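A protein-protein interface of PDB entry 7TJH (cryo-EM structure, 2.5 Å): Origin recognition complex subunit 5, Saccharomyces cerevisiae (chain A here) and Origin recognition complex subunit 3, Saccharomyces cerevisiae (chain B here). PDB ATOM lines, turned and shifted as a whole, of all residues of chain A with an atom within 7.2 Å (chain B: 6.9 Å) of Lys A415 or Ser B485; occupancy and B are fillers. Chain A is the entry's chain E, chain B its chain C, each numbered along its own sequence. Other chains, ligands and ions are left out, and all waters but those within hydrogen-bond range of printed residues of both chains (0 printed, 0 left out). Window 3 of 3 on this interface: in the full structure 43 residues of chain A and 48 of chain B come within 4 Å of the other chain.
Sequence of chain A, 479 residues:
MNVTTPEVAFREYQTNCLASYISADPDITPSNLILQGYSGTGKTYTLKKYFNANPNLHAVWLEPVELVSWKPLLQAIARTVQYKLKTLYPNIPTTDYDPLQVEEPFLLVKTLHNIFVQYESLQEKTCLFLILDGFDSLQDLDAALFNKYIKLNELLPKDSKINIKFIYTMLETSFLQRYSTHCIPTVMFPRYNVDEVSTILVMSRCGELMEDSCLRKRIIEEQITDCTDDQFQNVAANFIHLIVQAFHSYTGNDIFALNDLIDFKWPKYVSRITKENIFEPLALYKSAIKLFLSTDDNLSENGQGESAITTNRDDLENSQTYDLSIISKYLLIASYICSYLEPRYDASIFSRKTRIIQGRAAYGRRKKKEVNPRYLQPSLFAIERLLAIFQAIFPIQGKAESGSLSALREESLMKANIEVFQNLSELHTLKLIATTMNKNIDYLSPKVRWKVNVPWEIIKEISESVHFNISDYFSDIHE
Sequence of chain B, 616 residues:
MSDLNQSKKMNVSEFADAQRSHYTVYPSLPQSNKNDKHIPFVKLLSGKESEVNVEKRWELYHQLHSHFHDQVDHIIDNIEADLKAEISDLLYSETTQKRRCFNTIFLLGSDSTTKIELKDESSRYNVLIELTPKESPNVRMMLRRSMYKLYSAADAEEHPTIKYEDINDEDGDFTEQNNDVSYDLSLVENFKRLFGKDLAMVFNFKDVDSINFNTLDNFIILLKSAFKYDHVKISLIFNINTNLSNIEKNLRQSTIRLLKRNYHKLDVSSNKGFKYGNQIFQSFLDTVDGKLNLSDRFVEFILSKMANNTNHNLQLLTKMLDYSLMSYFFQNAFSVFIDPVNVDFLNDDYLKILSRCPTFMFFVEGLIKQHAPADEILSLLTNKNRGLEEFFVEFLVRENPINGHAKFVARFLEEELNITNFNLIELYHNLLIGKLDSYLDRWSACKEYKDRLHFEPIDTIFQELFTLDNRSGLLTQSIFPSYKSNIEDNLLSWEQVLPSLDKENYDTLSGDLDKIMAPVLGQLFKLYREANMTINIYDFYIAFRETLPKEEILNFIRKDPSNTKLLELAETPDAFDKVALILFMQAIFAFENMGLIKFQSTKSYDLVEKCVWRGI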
ATOM      1  N   PHE A 390     -13.684  23.315  18.024  1.00  0.00           N
ATOM      2  CA  PHE A 390     -13.898  24.757  18.141  1.00  0.00           C
ATOM      3  C   PHE A 390     -15.088  25.076  19.040  1.00  0.00           C
ATOM      4  O   PHE A 390     -15.032  26.016  19.838  1.00  0.00           O
ATOM      5  CB  PHE A 390     -14.096  25.365  16.749  1.00  0.00           C
ATOM      6  CG  PHE A 390     -14.578  26.796  16.759  1.00  0.00           C
ATOM      7  CD1 PHE A 390     -13.690  27.837  16.991  1.00  0.00           C
ATOM      8  CD2 PHE A 390     -15.910  27.101  16.511  1.00  0.00           C
ATOM      9  CE1 PHE A 390     -14.126  29.149  16.995  1.00  0.00           C
ATOM     10  CE2 PHE A 390     -16.350  28.411  16.519  1.00  0.00           C
ATOM     11  CZ  PHE A 390     -15.459  29.435  16.758  1.00  0.00           C
ATOM     12  N   GLN A 391     -16.178  24.312  18.914  1.00  0.00           N
ATOM     13  CA  GLN A 391     -17.322  24.507  19.796  1.00  0.00           C
ATOM     14  C   GLN A 391     -17.003  24.088  21.223  1.00  0.00           C
ATOM     15  O   GLN A 391     -17.516  24.689  22.173  1.00  0.00           O
ATOM     16  CB  GLN A 391     -18.529  23.727  19.271  1.00  0.00           C
ATOM     17  CG  GLN A 391     -19.859  24.189  19.833  1.00  0.00           C
ATOM     18  CD  GLN A 391     -21.015  23.327  19.373  1.00  0.00           C
ATOM     19  OE1 GLN A 391     -20.954  22.102  19.436  1.00  0.00           O
ATOM     20  NE2 GLN A 391     -22.075  23.967  18.897  1.00  0.00           N
ATOM     21  N   GLU A 411     -29.206  28.648  24.950  1.00  0.00           N
ATOM     22  CA  GLU A 411     -28.344  27.721  24.200  1.00  0.00           C
ATOM     23  C   GLU A 411     -26.958  28.332  23.964  1.00  0.00           C
ATOM     24  O   GLU A 411     -26.567  28.667  22.846  1.00  0.00           O
ATOM     25  CB  GLU A 411     -29.003  27.278  22.887  1.00  0.00           C
ATOM     26  CG  GLU A 411     -28.470  25.959  22.345  1.00  0.00           C
ATOM     27  CD  GLU A 411     -29.455  25.263  21.425  1.00  0.00           C
ATOM     28  OE1 GLU A 411     -30.623  25.698  21.364  1.00  0.00           O
ATOM     29  OE2 GLU A 411     -29.061  24.276  20.768  1.00  0.00           O
ATOM     30  N   SER A 412     -26.232  28.480  25.078  1.00  0.00           N
ATOM     31  CA  SER A 412     -25.031  29.309  25.165  1.00  0.00           C
ATOM     32  C   SER A 412     -23.861  28.816  24.318  1.00  0.00           C
ATOM     33  O   SER A 412     -22.901  29.574  24.139  1.00  0.00           O
ATOM     34  CB  SER A 412     -24.588  29.417  26.625  1.00  0.00           C
ATOM     35  OG  SER A 412     -25.651  29.859  27.449  1.00  0.00           O
ATOM     36  N   LEU A 413     -23.897  27.585  23.813  1.00  0.00           N
ATOM     37  CA  LEU A 413     -22.872  27.130  22.882  1.00  0.00           C
ATOM     38  C   LEU A 413     -22.999  27.852  21.547  1.00  0.00           C
ATOM     39  O   LEU A 413     -24.101  28.026  21.019  1.00  0.00           O
ATOM     40  CB  LEU A 413     -22.981  25.622  22.665  1.00  0.00           C
ATOM     41  CG  LEU A 413     -22.290  24.713  23.679  1.00  0.00           C
ATOM     42  CD1 LEU A 413     -22.355  23.278  23.202  1.00  0.00           C
ATOM     43  CD2 LEU A 413     -20.846  25.138  23.909  1.00  0.00           C
ATOM     44  N   MET A 414     -21.860  28.264  20.992  1.00  0.00           N
ATOM     45  CA  MET A 414     -21.850  28.955  19.709  1.00  0.00           C
ATOM     46  C   MET A 414     -21.907  27.939  18.578  1.00  0.00           C
ATOM     47  O   MET A 414     -21.055  27.050  18.487  1.00  0.00           O
ATOM     48  CB  MET A 414     -20.609  29.832  19.569  1.00  0.00           C
ATOM     49  CG  MET A 414     -20.825  31.044  18.682  1.00  0.00           C
ATOM     50  SD  MET A 414     -19.318  31.976  18.364  1.00  0.00           S
ATOM     51  CE  MET A 414     -19.545  32.431  16.651  1.00  0.00           C
ATOM     52  N   LYS A 415     -22.909  28.074  17.717  1.00  0.00           N
ATOM     53  CA  LYS A 415     -23.044  27.208  16.561  1.00  0.00           C
ATOM     54  C   LYS A 415     -22.287  27.794  15.371  1.00  0.00           C
ATOM     55  O   LYS A 415     -21.885  28.959  15.363  1.00  0.00           O
ATOM     56  CB  LYS A 415     -24.519  26.996  16.232  1.00  0.00           C
ATOM     57  CG  LYS A 415     -25.269  26.223  17.310  1.00  0.00           C
ATOM     58  CD  LYS A 415     -26.751  26.108  16.993  1.00  0.00           C
ATOM     59  CE  LYS A 415     -27.398  27.474  16.865  1.00  0.00           C
ATOM     60  NZ  LYS A 415     -28.846  27.372  16.538  1.00  0.00           N
ATOM     61  N   ALA A 416     -22.081  26.958  14.358  1.00  0.00           N
ATOM     62  CA  ALA A 416     -21.270  27.322  13.199  1.00  0.00           C
ATOM     63  C   ALA A 416     -22.115  28.142  12.231  1.00  0.00           C
ATOM     64  O   ALA A 416     -22.804  27.607  11.362  1.00  0.00           O
ATOM     65  CB  ALA A 416     -20.709  26.073  12.531  1.00  0.00           C
ATOM     66  N   ASN A 417     -22.065  29.461  12.388  1.00  0.00           N
ATOM     67  CA  ASN A 417     -22.762  30.374  11.496  1.00  0.00           C
ATOM     68  C   ASN A 417     -21.818  30.796  10.368  1.00  0.00           C
ATOM     69  O   ASN A 417     -20.739  30.226  10.193  1.00  0.00           O
ATOM     70  CB  ASN A 417     -23.320  31.556  12.286  1.00  0.00           C
ATOM     71  CG  ASN A 417     -22.241  32.465  12.835  1.00  0.00           C
ATOM     72  OD1 ASN A 417     -21.117  32.040  13.096  1.00  0.00           O
ATOM     73  ND2 ASN A 417     -22.589  33.727  13.031  1.00  0.00           N
ATOM     74  N   ILE A 418     -22.210  31.806   9.589  1.00  0.00           N
ATOM     75  CA  ILE A 418     -21.423  32.169   8.414  1.00  0.00           C
ATOM     76  C   ILE A 418     -20.154  32.937   8.766  1.00  0.00           C
ATOM     77  O   ILE A 418     -19.215  32.948   7.963  1.00  0.00           O
ATOM     78  CB  ILE A 418     -22.275  32.961   7.404  1.00  0.00           C
ATOM     79  CG1 ILE A 418     -22.792  34.272   8.006  1.00  0.00           C
ATOM     80  CG2 ILE A 418     -23.427  32.108   6.897  1.00  0.00           C
ATOM     81  CD1 ILE A 418     -22.116  35.525   7.482  1.00  0.00           C
ATOM     82  N   VAL A 420     -18.095  32.168  11.276  1.00  0.00           N
ATOM     83  CA  VAL A 420     -17.111  31.123  11.560  1.00  0.00           C
ATOM     84  C   VAL A 420     -16.530  30.567  10.262  1.00  0.00           C
ATOM     85  O   VAL A 420     -15.309  30.422  10.117  1.00  0.00           O
ATOM     86  CB  VAL A 420     -17.749  30.015  12.419  1.00  0.00           C
ATOM     87  CG1 VAL A 420     -16.845  28.788  12.509  1.00  0.00           C
ATOM     88  CG2 VAL A 420     -18.065  30.541  13.797  1.00  0.00           C
ATOM     89  N   PHE A 421     -17.399  30.277   9.288  1.00  0.00           N
ATOM     90  CA  PHE A 421     -16.942  29.749   8.006  1.00  0.00           C
ATOM     91  C   PHE A 421     -16.167  30.790   7.207  1.00  0.00           C
ATOM     92  O   PHE A 421     -15.213  30.441   6.504  1.00  0.00           O
ATOM     93  CB  PHE A 421     -18.132  29.229   7.200  1.00  0.00           C
ATOM     94  CG  PHE A 421     -18.604  27.875   7.635  1.00  0.00           C
ATOM     95  CD1 PHE A 421     -18.013  26.726   7.134  1.00  0.00           C
ATOM     96  CD2 PHE A 421     -19.637  27.748   8.549  1.00  0.00           C
ATOM     97  CE1 PHE A 421     -18.445  25.475   7.537  1.00  0.00           C
ATOM     98  CE2 PHE A 421     -20.075  26.502   8.958  1.00  0.00           C
ATOM     99  CZ  PHE A 421     -19.480  25.365   8.450  1.00  0.00           C
ATOM    100  N   SER B 482     -27.293  31.686  10.992  1.00  0.00           N
ATOM    101  CA  SER B 482     -26.838  30.357  11.388  1.00  0.00           C
ATOM    102  C   SER B 482     -27.269  29.385  10.294  1.00  0.00           C
ATOM    103  O   SER B 482     -28.236  28.634  10.432  1.00  0.00           O
ATOM    104  CB  SER B 482     -27.400  29.987  12.755  1.00  0.00           C
ATOM    105  OG  SER B 482     -28.583  29.220  12.638  1.00  0.00           O
ATOM    106  N   TYR B 483     -26.505  29.417   9.193  1.00  0.00           N
ATOM    107  CA  TYR B 483     -26.880  28.792   7.923  1.00  0.00           C
ATOM    108  C   TYR B 483     -27.046  27.282   8.061  1.00  0.00           C
ATOM    109  O   TYR B 483     -28.108  26.727   7.740  1.00  0.00           O
ATOM    110  CB  TYR B 483     -25.798  29.148   6.888  1.00  0.00           C
ATOM    111  CG  TYR B 483     -25.867  28.536   5.496  1.00  0.00           C
ATOM    112  CD1 TYR B 483     -25.367  27.256   5.232  1.00  0.00           C
ATOM    113  CD2 TYR B 483     -26.356  29.273   4.428  1.00  0.00           C
ATOM    114  CE1 TYR B 483     -25.415  26.717   3.970  1.00  0.00           C
ATOM    115  CE2 TYR B 483     -26.391  28.742   3.156  1.00  0.00           C
ATOM    116  CZ  TYR B 483     -25.926  27.465   2.933  1.00  0.00           C
ATOM    117  OH  TYR B 483     -25.967  26.931   1.670  1.00  0.00           O
ATOM    118  N   LYS B 484     -26.008  26.612   8.564  1.00  0.00           N
ATOM    119  CA  LYS B 484     -26.034  25.163   8.714  1.00  0.00           C
ATOM    120  C   LYS B 484     -27.052  24.738   9.765  1.00  0.00           C
ATOM    121  O   LYS B 484     -27.783  23.759   9.568  1.00  0.00           O
ATOM    122  CB  LYS B 484     -24.626  24.670   9.050  1.00  0.00           C
ATOM    123  CG  LYS B 484     -24.522  23.305   9.688  1.00  0.00           C
ATOM    124  CD  LYS B 484     -23.098  23.055  10.160  1.00  0.00           C
ATOM    125  CE  LYS B 484     -22.814  21.576  10.309  1.00  0.00           C
ATOM    126  NZ  LYS B 484     -23.232  21.083  11.653  1.00  0.00           N
ATOM    127  N   SER B 485     -27.152  25.500  10.858  1.00  0.00           N
ATOM    128  CA  SER B 485     -28.148  25.212  11.883  1.00  0.00           C
ATOM    129  C   SER B 485     -29.568  25.444  11.382  1.00  0.00           C
ATOM    130  O   SER B 485     -30.474  24.701  11.763  1.00  0.00           O
ATOM    131  CB  SER B 485     -27.879  26.053  13.130  1.00  0.00           C
ATOM    132  OG  SER B 485     -26.657  25.674  13.735  1.00  0.00           O
ATOM    133  N   ASN B 486     -29.779  26.448  10.520  1.00  0.00           N
ATOM    134  CA  ASN B 486     -31.101  26.648   9.925  1.00  0.00           C
ATOM    135  C   ASN B 486     -31.469  25.503   8.989  1.00  0.00           C
ATOM    136  O   ASN B 486     -32.625  25.063   8.976  1.00  0.00           O
ATOM    137  CB  ASN B 486     -31.165  27.980   9.175  1.00  0.00           C
ATOM    138  CG  ASN B 486     -31.301  29.169  10.105  1.00  0.00           C
ATOM    139  OD1 ASN B 486     -31.888  29.067  11.179  1.00  0.00           O
ATOM    140  ND2 ASN B 486     -30.755  30.306   9.694  1.00  0.00           N
ATOM    141  N   ILE B 487     -30.495  25.003   8.214  1.00  0.00           N
ATOM    142  CA  ILE B 487     -30.742  23.860   7.330  1.00  0.00           C
ATOM    143  C   ILE B 487     -31.113  22.622   8.146  1.00  0.00           C
ATOM    144  O   ILE B 487     -32.094  21.927   7.844  1.00  0.00           O
ATOM    145  CB  ILE B 487     -29.518  23.595   6.432  1.00  0.00           C
ATOM    146  CG1 ILE B 487     -29.306  24.734   5.429  1.00  0.00           C
ATOM    147  CG2 ILE B 487     -29.674  22.286   5.674  1.00  0.00           C
ATOM    148  CD1 ILE B 487     -30.396  24.864   4.396  1.00  0.00           C
ATOM    149  N   GLU B 488     -30.360  22.358   9.219  1.00  0.00           N
ATOM    150  CA  GLU B 488     -30.624  21.185  10.053  1.00  0.00           C
ATOM    151  C   GLU B 488     -31.938  21.314  10.818  1.00  0.00           C
ATOM    152  O   GLU B 488     -32.653  20.321  10.996  1.00  0.00           O
ATOM    153  CB  GLU B 488     -29.463  20.958  11.018  1.00  0.00           C
ATOM    154  CG  GLU B 488     -28.151  20.657  10.333  1.00  0.00           C
ATOM    155  CD  GLU B 488     -26.955  21.049  11.178  1.00  0.00           C
ATOM    156  OE1 GLU B 488     -27.052  22.030  11.945  1.00  0.00           O
ATOM    157  OE2 GLU B 488     -25.907  20.395  11.063  1.00  0.00           O
ATOM    158  N   ASP B 489     -32.274  22.527  11.273  1.00  0.00           N
ATOM    159  CA  ASP B 489     -33.530  22.760  11.979  1.00  0.00           C
ATOM    160  C   ASP B 489     -34.717  22.582  11.037  1.00  0.00           C
ATOM    161  O   ASP B 489     -35.732  21.988  11.419  1.00  0.00           O
ATOM    162  CB  ASP B 489     -33.497  24.168  12.595  1.00  0.00           C
ATOM    163  CG  ASP B 489     -34.840  24.634  13.177  1.00  0.00           C
ATOM    164  OD1 ASP B 489     -35.681  23.815  13.609  1.00  0.00           O
ATOM    165  OD2 ASP B 489     -35.051  25.864  13.209  1.00  0.00           O
ATOM    166  N   ASN B 490     -34.602  23.077   9.798  1.00  0.00           N
ATOM    167  CA  ASN B 490     -35.679  22.906   8.828  1.00  0.00           C
ATOM    168  C   ASN B 490     -35.822  21.450   8.406  1.00  0.00           C
ATOM    169  O   ASN B 490     -36.933  20.998   8.117  1.00  0.00           O
ATOM    170  CB  ASN B 490     -35.431  23.784   7.601  1.00  0.00           C
ATOM    171  CG  ASN B 490     -35.633  25.257   7.886  1.00  0.00           C
ATOM    172  OD1 ASN B 490     -36.543  25.644   8.618  1.00  0.00           O
ATOM    173  ND2 ASN B 490     -34.784  26.091   7.303  1.00  0.00           N
ATOM    174  N   LEU B 491     -34.711  20.711   8.355  1.00  0.00           N
ATOM    175  CA  LEU B 491     -34.771  19.289   8.033  1.00  0.00           C
ATOM    176  C   LEU B 491     -35.427  18.498   9.156  1.00  0.00           C
ATOM    177  O   LEU B 491     -36.290  17.648   8.913  1.00  0.00           O
ATOM    178  CB  LEU B 491     -33.361  18.763   7.763  1.00  0.00           C
ATOM    179  CG  LEU B 491     -32.802  18.907   6.351  1.00  0.00           C
ATOM    180  CD1 LEU B 491     -31.350  18.475   6.320  1.00  0.00           C
ATOM    181  CD2 LEU B 491     -33.622  18.104   5.358  1.00  0.00           C
ATOM    182  N   ARG B 614     -26.013  18.044  13.983  1.00  0.00           N
ATOM    183  CA  ARG B 614     -26.809  19.243  14.202  1.00  0.00           C
ATOM    184  C   ARG B 614     -26.330  19.999  15.436  1.00  0.00           C
ATOM    185  O   ARG B 614     -26.137  19.409  16.503  1.00  0.00           O
ATOM    186  CB  ARG B 614     -28.287  18.871  14.331  1.00  0.00           C
ATOM    187  CG  ARG B 614     -29.140  19.887  15.062  1.00  0.00           C
ATOM    188  CD  ARG B 614     -30.603  19.533  14.966  1.00  0.00           C
ATOM    189  NE  ARG B 614     -31.449  20.598  15.491  1.00  0.00           N
ATOM    190  CZ  ARG B 614     -32.012  20.582  16.690  1.00  0.00           C
ATOM    191  NH1 ARG B 614     -31.876  19.549  17.502  1.00  0.00           N
ATOM    192  NH2 ARG B 614     -32.742  21.623  17.078  1.00  0.00           N
ATOM    193  N   GLY B 615     -26.128  21.305  15.286  1.00  0.00           N
ATOM    194  CA  GLY B 615     -25.738  22.145  16.399  1.00  0.00           C
ATOM    195  C   GLY B 615     -24.253  22.256  16.640  1.00  0.00           C
ATOM    196  O   GLY B 615     -23.848  22.659  17.735  1.00  0.00           O
ATOM    197  N   ILE B 616     -23.425  21.900  15.661  1.00  0.00           N
ATOM    198  CA  ILE B 616     -21.977  21.903  15.834  1.00  0.00           C
ATOM    199  C   ILE B 616     -21.298  22.382  14.548  1.00  0.00           C
ATOM    200  O   ILE B 616     -21.604  21.921  13.449  1.00  0.00           O
ATOM    201  CB  ILE B 616     -21.473  20.500  16.261  1.00  0.00           C
ATOM    202  CG1 ILE B 616     -20.027  20.257  15.797  1.00  0.00           C
ATOM    203  CG2 ILE B 616     -22.434  19.431  15.768  1.00  0.00           C
ATOM    204  CD1 ILE B 616     -19.704  18.840  15.349  1.00  0.00           C
ATOM    205  OXT ILE B 616     -20.432  23.257  14.577  1.00  0.00           O
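NE2 of Gln A391 lies within hydrogen-bond range of O of Gly B615.
Gln A391 touches Ile B616 (OE1 to CB, 3.6 Å). Ser B485 touches Lys A415. Lys A415 touches Gly B615. Ala A416 touches Ile B616. Asn A417 touches Ser B482 (CB to CA, 3.8 Å). CG2 of Ile A418 touches CB of Tyr B483 (3.8 Å).
Hydrophobic or aromatic side chains of chain A that line the printed part of chain B: Ala A416 and Ile A418. Hydrophobic or aromatic side chains of chain B that line the printed part of chain A: Tyr B483 and Ile B616. Among the printed residues, no Asp or Glu carboxylate lies within 4 Å of a Lys or Arg side-chain nitrogen of the other chain.
Of the printed residues of chain B, Lys A415 touches Ser B485 and Gly B615. Of the printed residues of chain B, Gln A391 touches Gly B615 (2.5 Å) and Ile B616 (3.6 Å). Of the printed residues of chain A, Ile B616 touches Gln A391 (3.6 Å) and Ala A416 (3.5 Å). The nearest residue of chain B that does not touch Lys A415 is Ser B482 (4.3 Å). The nearest residue of chain A that does not touch Ser B485 is Ala A416 (4.8 Å). The nearest printed residue of chain A that does not touch Ser B482 is Lys A415 (4.3 Å).
The backbone carbonyl oxygen (O) of Met A414 lies within hydrogen-bond range of the side-chain amide nitrogen (NE2) of Gln A391 (3.3 Å). The side-chain amino group (NZ) of Lys B484 is in salt-bridge range of the chain-end carboxylate (O) of Ile B616 (2.6 Å). The backbone carbonyl oxygen (O) of Ser B482 lies within hydrogen-bond range of the side-chain amide nitrogen (ND2) of Asn B486 (3.1 Å).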
